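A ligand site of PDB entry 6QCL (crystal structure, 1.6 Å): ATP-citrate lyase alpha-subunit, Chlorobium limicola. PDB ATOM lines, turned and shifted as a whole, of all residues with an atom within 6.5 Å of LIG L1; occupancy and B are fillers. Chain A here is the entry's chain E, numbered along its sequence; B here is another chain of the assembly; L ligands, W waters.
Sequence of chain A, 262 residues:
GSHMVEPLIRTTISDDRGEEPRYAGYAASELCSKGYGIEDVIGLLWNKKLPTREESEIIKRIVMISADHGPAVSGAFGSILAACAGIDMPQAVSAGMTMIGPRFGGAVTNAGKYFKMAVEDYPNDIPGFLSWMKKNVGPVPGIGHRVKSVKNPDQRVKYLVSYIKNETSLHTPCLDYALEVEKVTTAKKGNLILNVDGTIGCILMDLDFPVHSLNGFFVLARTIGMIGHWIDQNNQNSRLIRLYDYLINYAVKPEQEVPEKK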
ATOM      1  N   GLY A 101       3.837   8.103  -4.612  1.00  0.00           N
ATOM      2  CA  GLY A 101       2.419   8.424  -4.652  1.00  0.00           C
ATOM      3  C   GLY A 101       2.159   9.888  -4.405  1.00  0.00           C
ATOM      4  O   GLY A 101       3.022  10.731  -4.634  1.00  0.00           O
ATOM      5  N   PRO A 102       0.983  10.219  -3.874  1.00  0.00           N
ATOM      6  CA  PRO A 102       0.624  11.639  -3.749  1.00  0.00           C
ATOM      7  C   PRO A 102       1.497  12.456  -2.819  1.00  0.00           C
ATOM      8  O   PRO A 102       1.761  13.615  -3.112  1.00  0.00           O
ATOM      9  CB  PRO A 102      -0.836  11.582  -3.266  1.00  0.00           C
ATOM     10  CG  PRO A 102      -0.950  10.264  -2.562  1.00  0.00           C
ATOM     11  CD  PRO A 102      -0.139   9.349  -3.463  1.00  0.00           C
ATOM     12  N   ARG A 103       2.052  11.826  -1.798  1.00  0.00           N
ATOM     13  CA  ARG A 103       2.899  12.550  -0.844  1.00  0.00           C
ATOM     14  C   ARG A 103       4.364  12.591  -1.221  1.00  0.00           C
ATOM     15  O   ARG A 103       5.048  13.602  -0.975  1.00  0.00           O
ATOM     16  CB  ARG A 103       2.737  11.954   0.546  1.00  0.00           C
ATOM     17  CG  ARG A 103       1.377  12.184   1.092  1.00  0.00           C
ATOM     18  CD  ARG A 103       1.185  11.581   2.454  1.00  0.00           C
ATOM     19  NE  ARG A 103      -0.116  11.928   2.984  1.00  0.00           N
ATOM     20  CZ  ARG A 103      -0.562  11.566   4.174  1.00  0.00           C
ATOM     21  NH1 ARG A 103      -1.754  11.983   4.603  1.00  0.00           N
ATOM     22  NH2 ARG A 103       0.170  10.798   4.970  1.00  0.00           N
ATOM     23  N   PHE A 104       4.870  11.475  -1.733  1.00  0.00           N
ATOM     24  CA  PHE A 104       6.254  11.304  -2.093  1.00  0.00           C
ATOM     25  C   PHE A 104       6.399  10.959  -3.552  1.00  0.00           C
ATOM     26  O   PHE A 104       6.036   9.869  -3.941  1.00  0.00           O
ATOM     27  CB  PHE A 104       6.869  10.178  -1.214  1.00  0.00           C
ATOM     28  CG  PHE A 104       8.189   9.643  -1.688  1.00  0.00           C
ATOM     29  CD1 PHE A 104       9.287  10.478  -1.811  1.00  0.00           C
ATOM     30  CD2 PHE A 104       8.320   8.338  -2.129  1.00  0.00           C
ATOM     31  CE1 PHE A 104      10.471  10.013  -2.383  1.00  0.00           C
ATOM     32  CE2 PHE A 104       9.502   7.886  -2.712  1.00  0.00           C
ATOM     33  CZ  PHE A 104      10.572   8.723  -2.816  1.00  0.00           C
ATOM     34  N   GLY A 105       6.998  11.868  -4.331  1.00  0.00           N
ATOM     35  CA  GLY A 105       7.403  11.589  -5.677  1.00  0.00           C
ATOM     36  C   GLY A 105       6.378  11.526  -6.779  1.00  0.00           C
ATOM     37  O   GLY A 105       6.738  11.831  -7.913  1.00  0.00           O
ATOM     38  N   GLY A 106       5.159  11.123  -6.492  1.00  0.00           N
ATOM     39  CA  GLY A 106       4.139  10.875  -7.522  1.00  0.00           C
ATOM     40  C   GLY A 106       3.087  11.939  -7.682  1.00  0.00           C
ATOM     41  O   GLY A 106       1.964  11.634  -8.096  1.00  0.00           O
ATOM     42  N   ALA A 107       3.428  13.179  -7.364  1.00  0.00           N
ATOM     43  CA  ALA A 107       2.537  14.329  -7.577  1.00  0.00           C
ATOM     44  C   ALA A 107       2.824  15.039  -8.905  1.00  0.00           C
ATOM     45  O   ALA A 107       2.172  16.046  -9.176  1.00  0.00           O
ATOM     46  CB  ALA A 107       2.720  15.330  -6.445  1.00  0.00           C
ATOM     47  N   ALA A 111       0.188  17.673 -10.565  1.00  0.00           N
ATOM     48  CA  ALA A 111       0.707  19.041 -10.578  1.00  0.00           C
ATOM     49  C   ALA A 111       0.629  19.637 -12.001  1.00  0.00           C
ATOM     50  O   ALA A 111       0.132  20.750 -12.202  1.00  0.00           O
ATOM     51  CB  ALA A 111       2.135  19.056 -10.062  1.00  0.00           C
ATOM     52  N   GLY A 138      -7.727  19.208  -2.503  1.00  0.00           N
ATOM     53  CA  GLY A 138      -7.031  19.085  -1.240  1.00  0.00           C
ATOM     54  C   GLY A 138      -5.700  19.803  -1.363  1.00  0.00           C
ATOM     55  O   GLY A 138      -5.657  20.851  -2.020  1.00  0.00           O
ATOM     56  N   PRO A 139      -4.583  19.265  -0.829  1.00  0.00           N
ATOM     57  CA  PRO A 139      -3.286  19.948  -0.993  1.00  0.00           C
ATOM     58  C   PRO A 139      -2.944  20.107  -2.460  1.00  0.00           C
ATOM     59  O   PRO A 139      -3.279  19.259  -3.286  1.00  0.00           O
ATOM     60  CB  PRO A 139      -2.270  19.043  -0.298  1.00  0.00           C
ATOM     61  CG  PRO A 139      -3.027  17.908   0.272  1.00  0.00           C
ATOM     62  CD  PRO A 139      -4.469  18.002  -0.069  1.00  0.00           C
ATOM     63  N   VAL A 140      -2.321  21.238  -2.793  1.00  0.00           N
ATOM     64  CA  VAL A 140      -1.955  21.542  -4.163  1.00  0.00           C
ATOM     65  C   VAL A 140      -0.810  20.644  -4.562  1.00  0.00           C
ATOM     66  O   VAL A 140       0.258  20.760  -3.966  1.00  0.00           O
ATOM     67  CB  VAL A 140      -1.592  23.027  -4.339  1.00  0.00           C
ATOM     68  CG1 VAL A 140      -1.140  23.337  -5.770  1.00  0.00           C
ATOM     69  CG2 VAL A 140      -2.768  23.927  -3.965  1.00  0.00           C
ATOM     70  N   PRO A 141      -0.976  19.728  -5.529  1.00  0.00           N
ATOM     71  CA  PRO A 141       0.175  18.918  -5.945  1.00  0.00           C
ATOM     72  C   PRO A 141       1.289  19.779  -6.526  1.00  0.00           C
ATOM     73  O   PRO A 141       1.011  20.715  -7.268  1.00  0.00           O
ATOM     74  CB  PRO A 141      -0.423  17.965  -6.981  1.00  0.00           C
ATOM     75  CG  PRO A 141      -1.911  18.024  -6.759  1.00  0.00           C
ATOM     76  CD  PRO A 141      -2.172  19.412  -6.339  1.00  0.00           C
ATOM     77  N   GLY A 142       2.530  19.456  -6.162  1.00  0.00           N
ATOM     78  CA  GLY A 142       3.689  20.180  -6.635  1.00  0.00           C
ATOM     79  C   GLY A 142       4.134  21.296  -5.744  1.00  0.00           C
ATOM     80  O   GLY A 142       5.112  21.981  -6.071  1.00  0.00           O
ATOM     81  N   ILE A 143       3.423  21.494  -4.633  1.00  0.00           N
ATOM     82  CA  ILE A 143       3.751  22.502  -3.621  1.00  0.00           C
ATOM     83  C   ILE A 143       4.013  21.762  -2.316  1.00  0.00           C
ATOM     84  O   ILE A 143       3.289  20.817  -1.984  1.00  0.00           O
ATOM     85  CB  ILE A 143       2.564  23.485  -3.453  1.00  0.00           C
ATOM     86  CG1 ILE A 143       2.329  24.328  -4.700  1.00  0.00           C
ATOM     87  CG2 ILE A 143       2.728  24.380  -2.240  1.00  0.00           C
ATOM     88  CD1 ILE A 143       3.398  25.469  -5.017  1.00  0.00           C
ATOM     89  N   GLY A 144       5.025  22.235  -1.598  1.00  0.00           N
ATOM     90  CA  GLY A 144       5.381  21.748  -0.259  1.00  0.00           C
ATOM     91  C   GLY A 144       6.523  20.769  -0.222  1.00  0.00           C
ATOM     92  O   GLY A 144       6.784  20.074  -1.194  1.00  0.00           O
ATOM     93  N   HIS A 145       7.190  20.663   0.917  1.00  0.00           N
ATOM     94  CA  HIS A 145       8.278  19.711   1.107  1.00  0.00           C
ATOM     95  C   HIS A 145       8.501  19.498   2.610  1.00  0.00           C
ATOM     96  O   HIS A 145       8.235  20.396   3.396  1.00  0.00           O
ATOM     97  CB  HIS A 145       9.583  20.217   0.459  1.00  0.00           C
ATOM     98  CG  HIS A 145      10.524  19.126   0.107  1.00  0.00           C
ATOM     99  ND1 HIS A 145      11.544  18.738   0.977  1.00  0.00           N
ATOM    100  CD2 HIS A 145      10.522  18.298  -0.964  1.00  0.00           C
ATOM    101  CE1 HIS A 145      12.144  17.707   0.384  1.00  0.00           C
ATOM    102  NE2 HIS A 145      11.559  17.400  -0.770  1.00  0.00           N
ATOM    103  N   ARG A 146       8.984  18.314   3.001  1.00  0.00           N
ATOM    104  CA  ARG A 146       9.269  18.058   4.419  1.00  0.00           C
ATOM    105  C   ARG A 146      10.508  18.836   4.909  1.00  0.00           C
ATOM    106  O   ARG A 146      10.532  19.262   6.094  1.00  0.00           O
ATOM    107  CB  ARG A 146       9.461  16.547   4.647  1.00  0.00           C
ATOM    108  CG  ARG A 146       9.895  16.165   6.059  1.00  0.00           C
ATOM    109  CD  ARG A 146       8.952  16.644   7.137  1.00  0.00           C
ATOM    110  NE  ARG A 146       7.625  16.064   7.007  1.00  0.00           N
ATOM    111  CZ  ARG A 146       7.286  14.819   7.355  1.00  0.00           C
ATOM    112  NH1 ARG A 146       6.041  14.385   7.183  1.00  0.00           N
ATOM    113  NH2 ARG A 146       8.200  13.986   7.846  1.00  0.00           N
ATOM    114  N   VAL A 147      11.560  18.977   4.061  1.00  0.00           N
ATOM    115  CA  VAL A 147      12.817  19.589   4.479  1.00  0.00           C
ATOM    116  C   VAL A 147      13.197  20.877   3.740  1.00  0.00           C
ATOM    117  O   VAL A 147      13.796  21.755   4.376  1.00  0.00           O
ATOM    118  CB  VAL A 147      13.968  18.555   4.450  1.00  0.00           C
ATOM    119  CG1 VAL A 147      13.704  17.439   5.464  1.00  0.00           C
ATOM    120  CG2 VAL A 147      14.193  17.934   3.090  1.00  0.00           C
ATOM    121  N   ARG A 156      17.718  21.945  -6.593  1.00  0.00           N
ATOM    122  CA  ARG A 156      17.329  21.172  -7.782  1.00  0.00           C
ATOM    123  C   ARG A 156      16.288  21.964  -8.538  1.00  0.00           C
ATOM    124  O   ARG A 156      16.349  22.020  -9.735  1.00  0.00           O
ATOM    125  CB  ARG A 156      16.752  19.816  -7.400  1.00  0.00           C
ATOM    126  CG  ARG A 156      17.740  18.857  -6.707  1.00  0.00           C
ATOM    127  CD  ARG A 156      17.052  17.614  -6.172  1.00  0.00           C
ATOM    128  NE  ARG A 156      16.039  17.930  -5.183  1.00  0.00           N
ATOM    129  CZ  ARG A 156      15.170  17.060  -4.688  1.00  0.00           C
ATOM    130  NH1 ARG A 156      15.227  15.782  -5.032  1.00  0.00           N
ATOM    131  NH2 ARG A 156      14.278  17.458  -3.798  1.00  0.00           N
ATOM    132  N   LYS A 189       3.179  30.323   4.275  1.00  0.00           N
ATOM    133  CA  LYS A 189       3.941  29.325   5.011  1.00  0.00           C
ATOM    134  C   LYS A 189       5.198  28.978   4.260  1.00  0.00           C
ATOM    135  O   LYS A 189       5.102  28.611   3.092  1.00  0.00           O
ATOM    136  CB  LYS A 189       3.092  28.052   5.178  1.00  0.00           C
ATOM    137  CG  LYS A 189       1.765  28.214   5.887  1.00  0.00           C
ATOM    138  CD  LYS A 189       1.035  26.872   5.978  1.00  0.00           C
ATOM    139  CE  LYS A 189      -0.386  27.008   6.495  1.00  0.00           C
ATOM    140  NZ  LYS A 189      -1.243  25.871   6.051  1.00  0.00           N
ATOM    141  N   ASN A 191       7.178  26.449   4.097  1.00  0.00           N
ATOM    142  CA  ASN A 191       7.361  25.108   3.538  1.00  0.00           C
ATOM    143  C   ASN A 191       6.656  24.977   2.164  1.00  0.00           C
ATOM    144  O   ASN A 191       6.903  23.995   1.492  1.00  0.00           O
ATOM    145  CB  ASN A 191       6.772  24.052   4.486  1.00  0.00           C
ATOM    146  CG  ASN A 191       5.333  24.316   4.860  1.00  0.00           C
ATOM    147  OD1 ASN A 191       5.055  25.336   5.494  1.00  0.00           O
ATOM    148  ND2 ASN A 191       4.385  23.450   4.493  1.00  0.00           N
ATOM    149  N   LEU A 192       5.759  25.911   1.776  1.00  0.00           N
ATOM    150  CA  LEU A 192       4.967  25.779   0.530  1.00  0.00           C
ATOM    151  C   LEU A 192       5.682  26.265  -0.733  1.00  0.00           C
ATOM    152  O   LEU A 192       5.159  27.020  -1.537  1.00  0.00           O
ATOM    153  CB  LEU A 192       3.621  26.467   0.678  1.00  0.00           C
ATOM    154  CG  LEU A 192       2.748  25.963   1.848  1.00  0.00           C
ATOM    155  CD1 LEU A 192       1.446  26.628   1.823  1.00  0.00           C
ATOM    156  CD2 LEU A 192       2.519  24.477   1.771  1.00  0.00           C
ATOM    157  N   ASN A 195       7.946  22.458  -5.457  1.00  0.00           N
ATOM    158  CA  ASN A 195       8.833  21.322  -5.255  1.00  0.00           C
ATOM    159  C   ASN A 195       9.242  20.703  -6.574  1.00  0.00           C
ATOM    160  O   ASN A 195       8.805  21.143  -7.648  1.00  0.00           O
ATOM    161  CB  ASN A 195       8.227  20.331  -4.245  1.00  0.00           C
ATOM    162  CG  ASN A 195       6.970  19.681  -4.717  1.00  0.00           C
ATOM    163  OD1 ASN A 195       6.874  19.273  -5.887  1.00  0.00           O
ATOM    164  ND2 ASN A 195       6.017  19.504  -3.802  1.00  0.00           N
ATOM    165  N   VAL A 196      10.085  19.670  -6.517  1.00  0.00           N
ATOM    166  CA  VAL A 196      10.583  19.048  -7.738  1.00  0.00           C
ATOM    167  C   VAL A 196       9.490  18.426  -8.562  1.00  0.00           C
ATOM    168  O   VAL A 196       9.496  18.543  -9.781  1.00  0.00           O
ATOM    169  CB  VAL A 196      11.745  18.065  -7.514  1.00  0.00           C
ATOM    170  CG1 VAL A 196      12.981  18.817  -7.089  1.00  0.00           C
ATOM    171  CG2 VAL A 196      11.402  16.977  -6.526  1.00  0.00           C
ATOM    172  N   ASP A 197       8.527  17.805  -7.907  1.00  0.00           N
ATOM    173  CA  ASP A 197       7.414  17.213  -8.655  1.00  0.00           C
ATOM    174  C   ASP A 197       6.646  18.332  -9.419  1.00  0.00           C
ATOM    175  O   ASP A 197       6.278  18.129 -10.548  1.00  0.00           O
ATOM    176  CB  ASP A 197       6.427  16.499  -7.733  1.00  0.00           C
ATOM    177  CG  ASP A 197       6.772  15.049  -7.387  1.00  0.00           C
ATOM    178  OD1 ASP A 197       7.716  14.476  -8.018  1.00  0.00           O
ATOM    179  OD2 ASP A 197       6.072  14.474  -6.543  1.00  0.00           O
ATOM    180  N   GLY A 198       6.380  19.474  -8.772  1.00  0.00           N
ATOM    181  CA  GLY A 198       5.684  20.573  -9.419  1.00  0.00           C
ATOM    182  C   GLY A 198       6.442  21.168 -10.596  1.00  0.00           C
ATOM    183  O   GLY A 198       5.884  21.455 -11.662  1.00  0.00           O
ATOM    184  N   PHE A 218       9.768  10.673 -12.617  1.00  0.00           N
ATOM    185  CA  PHE A 218      10.243  10.472 -11.241  1.00  0.00           C
ATOM    186  C   PHE A 218      10.384   8.959 -10.948  1.00  0.00           C
ATOM    187  O   PHE A 218      11.382   8.544 -10.346  1.00  0.00           O
ATOM    188  CB  PHE A 218       9.278  11.086 -10.252  1.00  0.00           C
ATOM    189  CG  PHE A 218       9.838  11.046  -8.855  1.00  0.00           C
ATOM    190  CD1 PHE A 218      10.688  12.045  -8.400  1.00  0.00           C
ATOM    191  CD2 PHE A 218       9.587   9.968  -8.017  1.00  0.00           C
ATOM    192  CE1 PHE A 218      11.231  12.000  -7.112  1.00  0.00           C
ATOM    193  CE2 PHE A 218      10.175   9.884  -6.760  1.00  0.00           C
ATOM    194  CZ  PHE A 218      10.984  10.911  -6.314  1.00  0.00           C
ATOM    195  N   ARG A 222      14.041   7.753  -9.940  1.00  0.00           N
ATOM    196  CA  ARG A 222      14.296   7.287  -8.568  1.00  0.00           C
ATOM    197  C   ARG A 222      14.581   5.790  -8.474  1.00  0.00           C
ATOM    198  O   ARG A 222      15.216   5.345  -7.523  1.00  0.00           O
ATOM    199  CB  ARG A 222      13.149   7.737  -7.639  1.00  0.00           C
ATOM    200  CG  ARG A 222      13.434   7.614  -6.173  1.00  0.00           C
ATOM    201  CD  ARG A 222      14.739   8.285  -5.682  1.00  0.00           C
ATOM    202  NE  ARG A 222      14.834   9.733  -6.007  1.00  0.00           N
ATOM    203  CZ  ARG A 222      14.363  10.729  -5.257  1.00  0.00           C
ATOM    204  NH1 ARG A 222      14.482  11.978  -5.648  1.00  0.00           N
ATOM    205  NH2 ARG A 222      13.805  10.481  -4.075  1.00  0.00           N
ATOM    206  N   ARG B 239       1.285  11.291   9.097  1.00  0.00           N
ATOM    207  CA  ARG B 239       2.000  12.007   8.036  1.00  0.00           C
ATOM    208  C   ARG B 239       3.135  11.176   7.493  1.00  0.00           C
ATOM    209  O   ARG B 239       3.562  10.202   8.089  1.00  0.00           O
ATOM    210  CB  ARG B 239       2.552  13.349   8.548  1.00  0.00           C
ATOM    211  CG  ARG B 239       1.483  14.292   9.050  1.00  0.00           C
ATOM    212  CD  ARG B 239       2.029  15.350  10.015  1.00  0.00           C
ATOM    213  NE  ARG B 239       3.105  16.176   9.431  1.00  0.00           N
ATOM    214  CZ  ARG B 239       4.402  16.105   9.731  1.00  0.00           C
ATOM    215  NH1 ARG B 239       5.270  16.934   9.153  1.00  0.00           N
ATOM    216  NH2 ARG B 239       4.860  15.209  10.606  1.00  0.00           N
ATOM    217  N   LEU B 240       3.668  11.616   6.361  1.00  0.00           N
ATOM    218  CA  LEU B 240       4.803  10.972   5.738  1.00  0.00           C
ATOM    219  C   LEU B 240       5.962  10.768   6.692  1.00  0.00           C
ATOM    220  O   LEU B 240       6.262  11.648   7.501  1.00  0.00           O
ATOM    221  CB  LEU B 240       5.252  11.867   4.580  1.00  0.00           C
ATOM    222  CG  LEU B 240       6.326  11.385   3.660  1.00  0.00           C
ATOM    223  CD1 LEU B 240       5.833  10.253   2.765  1.00  0.00           C
ATOM    224  CD2 LEU B 240       6.738  12.527   2.734  1.00  0.00           C
HETATM  225  N1  LIG L   1      -1.079  22.634  -0.373  1.00  0.00           N
HETATM  226  C1  LIG L   1      -1.634  23.241   0.676  1.00  0.00           C
HETATM  227  N2  LIG L   1      -1.274  23.172   1.968  1.00  0.00           N
HETATM  228  C2  LIG L   1      -0.204  22.370   2.130  1.00  0.00           C
HETATM  229  C3  LIG L   1       0.457  21.669   1.132  1.00  0.00           C
HETATM  230  C4  LIG L   1      -0.006  21.834  -0.182  1.00  0.00           C
HETATM  231  N3  LIG L   1       0.562  21.249  -1.227  1.00  0.00           N
HETATM  232  N4  LIG L   1       1.510  20.946   1.668  1.00  0.00           N
HETATM  233  C5  LIG L   1       1.472  21.225   2.950  1.00  0.00           C
HETATM  234  N5  LIG L   1       0.456  22.091   3.294  1.00  0.00           N
HETATM  235  C6  LIG L   1       0.165  22.606   4.631  1.00  0.00           C
HETATM  236  C7  LIG L   1      -0.640  21.623   5.471  1.00  0.00           C
HETATM  237  O1  LIG L   1      -2.021  21.910   5.300  1.00  0.00           O
HETATM  238  C8  LIG L   1      -0.112  21.935   6.861  1.00  0.00           C
HETATM  239  O2  LIG L   1      -0.694  23.184   7.305  1.00  0.00           O
HETATM  240  P1  LIG L   1      -1.141  23.403   8.863  1.00  0.00           P
HETATM  241  O3  LIG L   1       0.093  23.444   9.711  1.00  0.00           O
HETATM  242  O4  LIG L   1      -1.990  24.665   8.884  1.00  0.00           O
HETATM  243  O5  LIG L   1      -2.060  22.219   9.179  1.00  0.00           O
HETATM  244  C9  LIG L   1       1.367  22.208   6.603  1.00  0.00           C
HETATM  245  O6  LIG L   1       1.391  22.817   5.294  1.00  0.00           O
HETATM  246  C10 LIG L   1       2.280  21.017   6.620  1.00  0.00           C
HETATM  247  O7  LIG L   1       1.619  19.947   5.931  1.00  0.00           O
HETATM  248  P2  LIG L   1       1.796  18.380   6.286  1.00  0.00           P
HETATM  249  O8  LIG L   1       1.204  17.617   5.163  1.00  0.00           O
HETATM  250  O9  LIG L   1       1.324  18.161   7.720  1.00  0.00           O
HETATM  251  O10 LIG L   1       3.375  18.341   6.277  1.00  0.00           O
HETATM  252  P3  LIG L   1       4.438  17.454   5.510  1.00  0.00           P
HETATM  253  O11 LIG L   1       5.796  17.826   5.857  1.00  0.00           O
HETATM  254  O12 LIG L   1       4.096  16.013   5.812  1.00  0.00           O
HETATM  255  O13 LIG L   1       4.148  17.862   3.983  1.00  0.00           O
HETATM  256  C11 LIG L   1       4.233  17.009   1.720  1.00  0.00           C
HETATM  257  C12 LIG L   1       5.037  17.394   2.959  1.00  0.00           C
HETATM  258  C13 LIG L   1       3.663  15.591   1.940  1.00  0.00           C
HETATM  259  C14 LIG L   1       5.201  17.010   0.527  1.00  0.00           C
HETATM  260  C15 LIG L   1       3.074  17.995   1.445  1.00  0.00           C
HETATM  261  O14 LIG L   1       3.624  19.300   1.289  1.00  0.00           O
HETATM  262  C16 LIG L   1       2.167  17.621   0.275  1.00  0.00           C
HETATM  263  O15 LIG L   1       1.324  16.722   0.407  1.00  0.00           O
HETATM  264  N6  LIG L   1       2.358  18.282  -0.868  1.00  0.00           N
HETATM  265  C17 LIG L   1       1.594  18.030  -2.080  1.00  0.00           C
HETATM  266  C18 LIG L   1       2.033  16.757  -2.782  1.00  0.00           C
HETATM  267  C19 LIG L   1       3.403  16.890  -3.404  1.00  0.00           C
HETATM  268  O16 LIG L   1       3.639  17.840  -4.154  1.00  0.00           O
HETATM  269  N7  LIG L   1       4.294  15.944  -3.091  1.00  0.00           N
HETATM  270  C20 LIG L   1       5.647  15.895  -3.659  1.00  0.00           C
HETATM  271  C21 LIG L   1       6.735  16.464  -2.752  1.00  0.00           C
HETATM  272  S1  LIG L   1       8.277  16.649  -3.736  1.00  0.00           S
HETATM  273  C22 LIG L   1       8.724  14.953  -3.836  1.00  0.00           C
HETATM  274  O17 LIG L   1       8.289  14.132  -3.080  1.00  0.00           O
HETATM  275  C23 LIG L   1       9.885  14.708  -4.748  1.00  0.00           C
HETATM  276  C1  LG2 L   2      12.614  14.502  -3.023  1.00  0.00           C
HETATM  277  O1  LG2 L   2      12.364  15.677  -2.817  1.00  0.00           O
HETATM  278  O2  LG2 L   2      13.443  14.046  -3.919  1.00  0.00           O
HETATM  279  C2  LG2 L   2      11.962  13.378  -2.244  1.00  0.00           C
HETATM  280  O3  LG2 L   2      12.943  12.386  -2.035  1.00  0.00           O
HETATM  281  C3  LG2 L   2      11.279  13.872  -0.978  1.00  0.00           C
HETATM  282  C4  LG2 L   2      12.150  14.293   0.194  1.00  0.00           C
HETATM  283  O4  LG2 L   2      13.435  14.374  -0.062  1.00  0.00           O
HETATM  284  O5  LG2 L   2      11.680  14.520   1.309  1.00  0.00           O
HETATM  285  O   HOH W   1      -0.067  15.868   2.567  1.00  0.00           O
HETATM  286  O   HOH W   2       0.051  15.226   5.125  1.00  0.00           O
HETATM  287  O   HOH W   3       6.321  20.458   5.583  1.00  0.00           O
HETATM  288  O   HOH W   4       2.474  13.963   5.105  1.00  0.00           O
HETATM  289  O   HOH W   5      -0.504  15.131  -0.888  1.00  0.00           O
HETATM  290  O   HOH W   6      -0.242  15.008  -4.694  1.00  0.00           O
HETATM  291  O   HOH W   7      -2.275  25.192   3.577  1.00  0.00           O
HETATM  292  O   HOH W   8       4.863  21.081   3.097  1.00  0.00           O
HETATM  293  O   HOH W   9       7.850  13.977  -0.184  1.00  0.00           O
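Water W3 lies within hydrogen-bond range of O11 of LIG L1 (2.7 Å) and O of His 145 (2.9 Å).
Water W4 bridges O12 of LIG L1 and N of Leu 240 of chain B.
Water W7 lies within hydrogen-bond range of the side-chain amino group (NZ) of Lys 189 (2.8 Å) and a nitrogen (N2) of LIG L1 (2.8 Å).
Water W8 lies within hydrogen-bond range of the side-chain amide nitrogen of Asn 191 (2.8 Å), an oxygen (O14) of LIG L1 (2.8 Å) and the backbone NH of His 145 (3.2 Å).
Water W9 lies within hydrogen-bond range of O17 of LIG L1 (2.9 Å) and O of Arg 103 (2.9 Å).
NE of Arg 146 is in salt-bridge range of O11 of LIG L1, 2.8 Å away.
N of Val 140 is in hydrogen-bond range of N1 of LIG L1.
O of Val 140 sits at hydrogen-bond distance from N3 of LIG L1 (2.8 Å).
The backbone NH of Gly 142 is in hydrogen-bond range of an oxygen (O16) of LIG L1.
N3 of LIG L1 sits at hydrogen-bond distance from O of Ile 143 (2.9 Å).
The backbone NH (N) of Gly 105 lies within hydrogen-bond range of an oxygen (O17) of LIG L1 (2.9 Å).
ND2 of Asn 195 sits at hydrogen-bond distance from O16 of LIG L1 (2.9 Å).
O4 of LIG L1 is in salt-bridge range of NZ of Lys 189, at 3.2 Å.
The side-chain amide nitrogen (ND2) of Asn 191 lies within hydrogen-bond range of an oxygen (O6) of LIG L1, 3.2 Å away.
The guanidinium group of Arg 239 of chain B is in salt-bridge range of an oxygen (O9) of LIG L1 (3.2 Å).
A nitrogen (N7) of LIG L1 sits close to the backbone carbonyl oxygen (O) of Pro 102, 3.4 Å away.
The backbone carbonyl oxygen (O) of Arg 103 lies within hydrogen-bond range of a nitrogen (N7) of LIG L1.
O1 of LG2 L2 lies within hydrogen-bond range of NE2 of His 145.
O2 of LG2 L2 is in salt-bridge range of NH1 of Arg 156 (2.7 Å).
The guanidinium group of Arg 222 is in salt-bridge range of an oxygen (O2) of LG2 L2, 2.9 Å away.
Phe 104 touches LIG L1.
CB of Ala 107 touches C19 of LIG L1, at 3.5 Å.
CA of Pro 139 touches N1 of LIG L1, at 3.5 Å.
C of Pro 141 touches O16 of LIG L1, 3.9 Å away.
CA of Gly 144 touches O14 of LIG L1 (3.4 Å).
His 145 touches LIG L1.
Leu 192 touches LIG L1.
Val 196 touches LIG L1 (CG2 to C23, 3.3 Å).
OD2 of Asp 197 touches C20 of LIG L1, at 3.2 Å.
Phe 218 touches LIG L1 (CE1 to C23, 3.8 Å).
21 residues have an atom within 4 Å of LIG L1: Pro 102, Arg 103, Phe 104, Gly 105, Ala 107, Pro 139, Val 140, Pro 141, Gly 142, Ile 143, Gly 144, His 145, Arg 146, Lys 189, Asn 191, Leu 192, Asn 195, Val 196, Asp 197, Phe 218 and Arg 239 of chain B.
Along chain A the residues within 4 Å of LIG L1 span positions 102 to 218.
The nearest printed residue that does not touch LIG L1 is Leu 240 of chain B (4.4 Å).
N of Asn 195 sits at hydrogen-bond distance from O of Gly 142 (2.9 Å).
OD1 of Asn 195 lies within hydrogen-bond range of N of Asp 197 (3.0 Å).
The backbone carbonyl oxygen of Gly 144 sits at hydrogen-bond distance from the side-chain amide nitrogen of Asn 195, at 2.8 Å.
The side-chain amide oxygen (OD1) of Asn 195 is in hydrogen-bond range of the backbone NH (N) of Gly 198 (2.9 Å).
N of His 145 lies within hydrogen-bond range of O of Asn 191 (3.4 Å).
The side-chain carboxylate (OD2) of Asp 197 sits at hydrogen-bond distance from the backbone NH (N) of Ala 107.
N of Gly 106 lies within hydrogen-bond range of OD2 of Asp 197, at 3.5 Å.
A ring nitrogen (ND1) of His 145 is in hydrogen-bond range of the backbone NH (N) of Val 147 (3.1 Å).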
